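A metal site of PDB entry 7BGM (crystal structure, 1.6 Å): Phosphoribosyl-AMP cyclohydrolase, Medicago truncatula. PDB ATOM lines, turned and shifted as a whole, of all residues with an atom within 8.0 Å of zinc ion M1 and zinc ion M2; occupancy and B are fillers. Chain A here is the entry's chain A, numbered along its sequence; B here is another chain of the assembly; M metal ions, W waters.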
ATOM      1  N   LEU A  32      -3.869 -36.036  -9.319  1.00  0.00           N
ATOM      2  CA  LEU A  32      -3.497 -35.606 -10.655  1.00  0.00           C
ATOM      3  C   LEU A  32      -4.393 -34.486 -11.158  1.00  0.00           C
ATOM      4  O   LEU A  32      -3.903 -33.514 -11.767  1.00  0.00           O
ATOM      5  CB  LEU A  32      -3.596 -36.807 -11.616  1.00  0.00           C
ATOM      6  CG  LEU A  32      -2.747 -38.024 -11.194  1.00  0.00           C
ATOM      7  CD1 LEU A  32      -2.986 -39.251 -12.105  1.00  0.00           C
ATOM      8  CD2 LEU A  32      -1.264 -37.650 -11.153  1.00  0.00           C
ATOM      9  N   MET A  33      -5.707 -34.662 -10.989  1.00  0.00           N
ATOM     10  CA  MET A  33      -6.690 -33.705 -11.521  1.00  0.00           C
ATOM     11  C   MET A  33      -8.043 -34.070 -10.919  1.00  0.00           C
ATOM     12  O   MET A  33      -8.233 -35.189 -10.423  1.00  0.00           O
ATOM     13  CB  MET A  33      -6.793 -33.728 -13.070  1.00  0.00           C
ATOM     14  CG  MET A  33      -7.266 -35.092 -13.588  1.00  0.00           C
ATOM     15  SD  MET A  33      -7.573 -35.133 -15.370  1.00  0.00           S
ATOM     16  CE  MET A  33      -9.088 -34.178 -15.492  1.00  0.00           C
ATOM     17  N   GLN A  34      -8.983 -33.129 -11.016  1.00  0.00           N
ATOM     18  CA  GLN A  34     -10.326 -33.409 -10.564  1.00  0.00           C
ATOM     19  C   GLN A  34     -11.280 -32.816 -11.586  1.00  0.00           C
ATOM     20  O   GLN A  34     -11.059 -31.696 -12.072  1.00  0.00           O
ATOM     21  CB  GLN A  34     -10.594 -32.836  -9.155  1.00  0.00           C
ATOM     22  CG  GLN A  34     -12.076 -32.931  -8.701  1.00  0.00           C
ATOM     23  CD  GLN A  34     -12.865 -31.629  -8.952  1.00  0.00           C
ATOM     24  OE1 GLN A  34     -12.496 -30.561  -8.459  1.00  0.00           O
ATOM     25  NE2 GLN A  34     -13.941 -31.723  -9.719  1.00  0.00           N
ATOM     26  N   TRP A  62     -14.935 -36.588 -22.465  1.00  0.00           N
ATOM     27  CA  TRP A  62     -13.564 -36.527 -22.943  1.00  0.00           C
ATOM     28  C   TRP A  62     -12.694 -37.421 -22.081  1.00  0.00           C
ATOM     29  O   TRP A  62     -12.922 -37.593 -20.882  1.00  0.00           O
ATOM     30  CB  TRP A  62     -12.987 -35.102 -22.963  1.00  0.00           C
ATOM     31  CG  TRP A  62     -12.783 -34.481 -21.606  1.00  0.00           C
ATOM     32  CD1 TRP A  62     -13.753 -33.972 -20.751  1.00  0.00           C
ATOM     33  CD2 TRP A  62     -11.524 -34.243 -20.971  1.00  0.00           C
ATOM     34  NE1 TRP A  62     -13.146 -33.447 -19.611  1.00  0.00           N
ATOM     35  CE2 TRP A  62     -11.787 -33.591 -19.735  1.00  0.00           C
ATOM     36  CE3 TRP A  62     -10.198 -34.486 -21.345  1.00  0.00           C
ATOM     37  CZ2 TRP A  62     -10.759 -33.211 -18.849  1.00  0.00           C
ATOM     38  CZ3 TRP A  62      -9.177 -34.096 -20.487  1.00  0.00           C
ATOM     39  CH2 TRP A  62      -9.468 -33.485 -19.229  1.00  0.00           C
ATOM     40  N   LYS A  64      -8.953 -38.120 -20.687  1.00  0.00           N
ATOM     41  CA  LYS A  64      -7.675 -37.470 -20.450  1.00  0.00           C
ATOM     42  C   LYS A  64      -6.601 -38.161 -21.274  1.00  0.00           C
ATOM     43  O   LYS A  64      -6.462 -39.394 -21.227  1.00  0.00           O
ATOM     44  CB  LYS A  64      -7.354 -37.520 -18.965  1.00  0.00           C
ATOM     45  CG  LYS A  64      -5.971 -37.099 -18.641  1.00  0.00           C
ATOM     46  CD  LYS A  64      -5.797 -35.606 -18.941  1.00  0.00           C
ATOM     47  CE  LYS A  64      -4.439 -35.289 -19.471  1.00  0.00           C
ATOM     48  NZ  LYS A  64      -4.353 -33.801 -19.739  1.00  0.00           N
ATOM     49  N   THR A  96      -0.118 -34.602 -16.274  1.00  0.00           N
ATOM     50  CA  THR A  96      -1.560 -34.600 -16.440  1.00  0.00           C
ATOM     51  C   THR A  96      -2.094 -33.235 -16.858  1.00  0.00           C
ATOM     52  O   THR A  96      -3.111 -33.160 -17.553  1.00  0.00           O
ATOM     53  CB  THR A  96      -2.209 -35.046 -15.112  1.00  0.00           C
ATOM     54  OG1 THR A  96      -1.830 -36.411 -14.830  1.00  0.00           O
ATOM     55  CG2 THR A  96      -3.738 -34.913 -15.158  1.00  0.00           C
ATOM     56  N   CYS A  97      -1.428 -32.147 -16.458  1.00  0.00           N
ATOM     57  CA  CYS A  97      -1.998 -30.823 -16.698  1.00  0.00           C
ATOM     58  C   CYS A  97      -1.672 -30.335 -18.114  1.00  0.00           C
ATOM     59  O   CYS A  97      -0.576 -30.574 -18.636  1.00  0.00           O
ATOM     60  CB  CYS A  97      -1.518 -29.802 -15.635  1.00  0.00           C
ATOM     61  SG  CYS A  97      -2.423 -28.221 -15.780  1.00  0.00           S
ATOM     62  N   HIS A  98      -2.651 -29.696 -18.752  1.00  0.00           N
ATOM     63  CA  HIS A  98      -2.448 -29.099 -20.063  1.00  0.00           C
ATOM     64  C   HIS A  98      -1.330 -28.073 -20.066  1.00  0.00           C
ATOM     65  O   HIS A  98      -0.760 -27.778 -21.127  1.00  0.00           O
ATOM     66  CB  HIS A  98      -3.740 -28.441 -20.560  1.00  0.00           C
ATOM     67  CG  HIS A  98      -4.166 -27.252 -19.739  1.00  0.00           C
ATOM     68  ND1 HIS A  98      -3.845 -25.956 -20.073  1.00  0.00           N
ATOM     69  CD2 HIS A  98      -4.894 -27.179 -18.598  1.00  0.00           C
ATOM     70  CE1 HIS A  98      -4.344 -25.129 -19.170  1.00  0.00           C
ATOM     71  NE2 HIS A  98      -4.993 -25.837 -18.263  1.00  0.00           N
ATOM     72  N   THR A  99      -1.014 -27.496 -18.906  1.00  0.00           N
ATOM     73  CA  THR A  99       0.080 -26.535 -18.813  1.00  0.00           C
ATOM     74  C   THR A  99       1.441 -27.209 -18.881  1.00  0.00           C
ATOM     75  O   THR A  99       2.458 -26.514 -18.977  1.00  0.00           O
ATOM     76  CB  THR A  99       0.021 -25.750 -17.494  1.00  0.00           C
ATOM     77  OG1 THR A  99       0.205 -26.647 -16.388  1.00  0.00           O
ATOM     78  CG2 THR A  99      -1.297 -25.007 -17.341  1.00  0.00           C
ATOM     79  N   GLY A 100       1.500 -28.545 -18.813  1.00  0.00           N
ATOM     80  CA  GLY A 100       2.751 -29.274 -18.741  1.00  0.00           C
ATOM     81  C   GLY A 100       3.158 -29.697 -17.338  1.00  0.00           C
ATOM     82  O   GLY A 100       4.050 -30.558 -17.204  1.00  0.00           O
ATOM     83  N   ALA A 101       2.529 -29.134 -16.308  1.00  0.00           N
ATOM     84  CA  ALA A 101       2.804 -29.534 -14.931  1.00  0.00           C
ATOM     85  C   ALA A 101       2.408 -30.985 -14.701  1.00  0.00           C
ATOM     86  O   ALA A 101       1.488 -31.503 -15.326  1.00  0.00           O
ATOM     87  CB  ALA A 101       2.026 -28.651 -13.953  1.00  0.00           C
ATOM     88  N   GLU A 102       3.099 -31.643 -13.771  1.00  0.00           N
ATOM     89  CA  GLU A 102       2.878 -33.060 -13.555  1.00  0.00           C
ATOM     90  C   GLU A 102       1.456 -33.356 -13.073  1.00  0.00           C
ATOM     91  O   GLU A 102       0.856 -34.373 -13.442  1.00  0.00           O
ATOM     92  CB  GLU A 102       3.920 -33.563 -12.557  1.00  0.00           C
ATOM     93  CG  GLU A 102       4.007 -34.997 -12.468  1.00  0.00           C
ATOM     94  CD  GLU A 102       5.304 -35.395 -11.813  1.00  0.00           C
ATOM     95  OE1 GLU A 102       6.375 -35.035 -12.344  1.00  0.00           O
ATOM     96  OE2 GLU A 102       5.241 -36.003 -10.756  1.00  0.00           O
ATOM     97  N   THR A 103       0.923 -32.453 -12.257  1.00  0.00           N
ATOM     98  CA  THR A 103      -0.465 -32.476 -11.808  1.00  0.00           C
ATOM     99  C   THR A 103      -1.043 -31.100 -12.001  1.00  0.00           C
ATOM    100  O   THR A 103      -0.317 -30.113 -12.236  1.00  0.00           O
ATOM    101  CB  THR A 103      -0.633 -32.834 -10.317  1.00  0.00           C
ATOM    102  OG1 THR A 103      -0.234 -31.687  -9.533  1.00  0.00           O
ATOM    103  CG2 THR A 103       0.228 -34.082  -9.954  1.00  0.00           C
ATOM    104  N   CYS A 104      -2.346 -31.038 -11.850  1.00  0.00           N
ATOM    105  CA  CYS A 104      -3.008 -29.746 -11.994  1.00  0.00           C
ATOM    106  C   CYS A 104      -2.867 -28.847 -10.742  1.00  0.00           C
ATOM    107  O   CYS A 104      -3.323 -27.697 -10.775  1.00  0.00           O
ATOM    108  CB  CYS A 104      -4.493 -29.931 -12.322  1.00  0.00           C
ATOM    109  SG  CYS A 104      -4.829 -30.645 -13.941  1.00  0.00           S
ATOM    110  N   TYR A 105      -2.222 -29.307  -9.684  1.00  0.00           N
ATOM    111  CA  TYR A 105      -2.219 -28.608  -8.381  1.00  0.00           C
ATOM    112  C   TYR A 105      -0.823 -28.122  -8.072  1.00  0.00           C
ATOM    113  O   TYR A 105       0.014 -28.884  -7.566  1.00  0.00           O
ATOM    114  CB  TYR A 105      -2.765 -29.501  -7.251  1.00  0.00           C
ATOM    115  CG  TYR A 105      -4.213 -29.912  -7.440  1.00  0.00           C
ATOM    116  CD1 TYR A 105      -5.256 -29.133  -6.896  1.00  0.00           C
ATOM    117  CD2 TYR A 105      -4.560 -31.036  -8.211  1.00  0.00           C
ATOM    118  CE1 TYR A 105      -6.584 -29.514  -7.057  1.00  0.00           C
ATOM    119  CE2 TYR A 105      -5.887 -31.411  -8.395  1.00  0.00           C
ATOM    120  CZ  TYR A 105      -6.897 -30.647  -7.807  1.00  0.00           C
ATOM    121  OH  TYR A 105      -8.209 -31.052  -8.003  1.00  0.00           O
ATOM    122  N   TYR A 106      -0.561 -26.869  -8.425  1.00  0.00           N
ATOM    123  CA  TYR A 106       0.740 -26.232  -8.254  1.00  0.00           C
ATOM    124  C   TYR A 106       0.604 -24.768  -7.811  1.00  0.00           C
ATOM    125  O   TYR A 106       1.573 -23.987  -7.924  1.00  0.00           O
ATOM    126  CB  TYR A 106       1.525 -26.320  -9.571  1.00  0.00           C
ATOM    127  CG  TYR A 106       0.744 -25.853 -10.746  1.00  0.00           C
ATOM    128  CD1 TYR A 106       0.635 -24.484 -11.019  1.00  0.00           C
ATOM    129  CD2 TYR A 106       0.143 -26.757 -11.622  1.00  0.00           C
ATOM    130  CE1 TYR A 106      -0.072 -24.026 -12.099  1.00  0.00           C
ATOM    131  CE2 TYR A 106      -0.590 -26.319 -12.722  1.00  0.00           C
ATOM    132  CZ  TYR A 106      -0.689 -24.945 -12.955  1.00  0.00           C
ATOM    133  OH  TYR A 106      -1.405 -24.436 -14.017  1.00  0.00           O
ATOM    134  N   LYS B  12     -12.449 -19.530  -9.251  1.00  0.00           N
ATOM    135  CA  LYS B  12     -13.545 -19.706 -10.199  1.00  0.00           C
ATOM    136  C   LYS B  12     -14.688 -20.434  -9.487  1.00  0.00           C
ATOM    137  O   LYS B  12     -14.871 -21.651  -9.608  1.00  0.00           O
ATOM    138  CB  LYS B  12     -13.052 -20.467 -11.428  1.00  0.00           C
ATOM    139  CG  LYS B  12     -14.083 -20.694 -12.526  1.00  0.00           C
ATOM    140  CD  LYS B  12     -13.434 -21.288 -13.771  1.00  0.00           C
ATOM    141  CE  LYS B  12     -14.340 -22.293 -14.489  1.00  0.00           C
ATOM    142  NZ  LYS B  12     -13.681 -23.645 -14.569  1.00  0.00           N
ATOM    143  N   ASP B  80      -6.228 -25.780  -8.190  1.00  0.00           N
ATOM    144  CA  ASP B  80      -5.861 -26.396  -9.466  1.00  0.00           C
ATOM    145  C   ASP B  80      -5.705 -25.339 -10.554  1.00  0.00           C
ATOM    146  O   ASP B  80      -5.913 -24.137 -10.337  1.00  0.00           O
ATOM    147  CB  ASP B  80      -6.819 -27.540  -9.827  1.00  0.00           C
ATOM    148  CG  ASP B  80      -8.126 -27.105 -10.446  1.00  0.00           C
ATOM    149  OD1 ASP B  80      -8.516 -25.946 -10.154  1.00  0.00           O
ATOM    150  OD2 ASP B  80      -8.765 -27.963 -11.185  1.00  0.00           O
ATOM    151  N   CYS B  81      -5.297 -25.793 -11.749  1.00  0.00           N
ATOM    152  CA  CYS B  81      -4.848 -24.868 -12.811  1.00  0.00           C
ATOM    153  C   CYS B  81      -5.933 -23.876 -13.232  1.00  0.00           C
ATOM    154  O   CYS B  81      -5.625 -22.723 -13.581  1.00  0.00           O
ATOM    155  CB  CYS B  81      -4.390 -25.691 -14.024  1.00  0.00           C
ATOM    156  SG  CYS B  81      -5.673 -26.821 -14.688  1.00  0.00           S
ATOM    157  N   ASP B  82      -7.206 -24.303 -13.267  1.00  0.00           N
ATOM    158  CA  ASP B  82      -8.292 -23.379 -13.623  1.00  0.00           C
ATOM    159  C   ASP B  82      -9.046 -22.845 -12.418  1.00  0.00           C
ATOM    160  O   ASP B  82     -10.057 -22.116 -12.582  1.00  0.00           O
ATOM    161  CB  ASP B  82      -9.257 -24.011 -14.653  1.00  0.00           C
ATOM    162  CG  ASP B  82      -9.881 -25.323 -14.184  1.00  0.00           C
ATOM    163  OD1 ASP B  82      -9.639 -25.785 -13.042  1.00  0.00           O
ATOM    164  OD2 ASP B  82     -10.637 -25.909 -15.014  1.00  0.00           O
ATOM    165  N   ARG B  83      -8.542 -23.133 -11.204  1.00  0.00           N
ATOM    166  CA  ARG B  83      -8.921 -22.440  -9.955  1.00  0.00           C
ATOM    167  C   ARG B  83     -10.349 -22.749  -9.503  1.00  0.00           C
ATOM    168  O   ARG B  83     -10.972 -21.939  -8.799  1.00  0.00           O
ATOM    169  CB  ARG B  83      -8.690 -20.916 -10.081  1.00  0.00           C
ATOM    170  CG  ARG B  83      -7.349 -20.546 -10.734  1.00  0.00           C
ATOM    171  CD  ARG B  83      -7.153 -19.061 -10.903  1.00  0.00           C
ATOM    172  NE  ARG B  83      -6.754 -18.419  -9.674  1.00  0.00           N
ATOM    173  CZ  ARG B  83      -5.504 -18.354  -9.206  1.00  0.00           C
ATOM    174  NH1 ARG B  83      -4.479 -18.969  -9.833  1.00  0.00           N
ATOM    175  NH2 ARG B  83      -5.270 -17.683  -8.085  1.00  0.00           N
ATOM    176  N   ASP B  84     -10.884 -23.930  -9.841  1.00  0.00           N
ATOM    177  CA  ASP B  84     -12.200 -24.346  -9.324  1.00  0.00           C
ATOM    178  C   ASP B  84     -12.116 -25.536  -8.386  1.00  0.00           C
ATOM    179  O   ASP B  84     -13.157 -26.079  -7.985  1.00  0.00           O
ATOM    180  CB  ASP B  84     -13.185 -24.650 -10.475  1.00  0.00           C
ATOM    181  CG  ASP B  84     -12.672 -25.696 -11.399  1.00  0.00           C
ATOM    182  OD1 ASP B  84     -11.639 -26.290 -11.056  1.00  0.00           O
ATOM    183  OD2 ASP B  84     -13.242 -25.915 -12.486  1.00  0.00           O
HETATM  184 ZN    ZN M   1      -4.549 -28.768 -15.256  1.00  0.00          ZN
HETATM  185 ZN    ZN M   2      -6.256 -25.452 -16.725  1.00  0.00          ZN
HETATM  186 ZN    ZN M   3     -10.380 -27.422 -12.157  1.00  0.00          ZN
HETATM  187  O   HOH W   1      -5.398 -23.057 -16.454  1.00  0.00           O
HETATM  188  O   HOH W   2      -8.348 -25.519 -17.275  1.00  0.00           O
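Merely in contact with zinc ion M2: Asp 82 of chain B (3.8 Å).
Three residues have an atom within 4 Å of zinc ion M2: His 98, Cys 81 of chain B and Asp 82 of chain B.
OG1 of Thr 99 sits close to SG of Cys 97, at 3.1 Å.
The side-chain amino group (NZ) of Lys 12 of chain B is in salt-bridge range of the side-chain carboxylate (OD2) of Asp 82 of chain B (3.8 Å).
The backbone NH (N) of Cys 104 sits at hydrogen-bond distance from the backbone carbonyl oxygen (O) of Leu 32, at 2.9 Å.
Zinc ion M2 is bound by NE2 of His 98, 2.0 Å away.
Water W2 is bound to zinc ion M2 (2.2 Å).
Zinc ion M2 is bound by SG of Cys 81 of chain B (2.5 Å).
Water W1 is bound to zinc ion M2, 2.6 Å away.
Zinc ion M2 has four donor atoms within binding distance.
Zinc ion M1 is bound by the side-chain sulfur (SG) of Cys 97.
Zinc ion M1 is bound by SG of Cys 104 (2.3 Å).
The side-chain sulfur (SG) of Cys 81 of chain B is bound to zinc ion M1 (2.3 Å).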
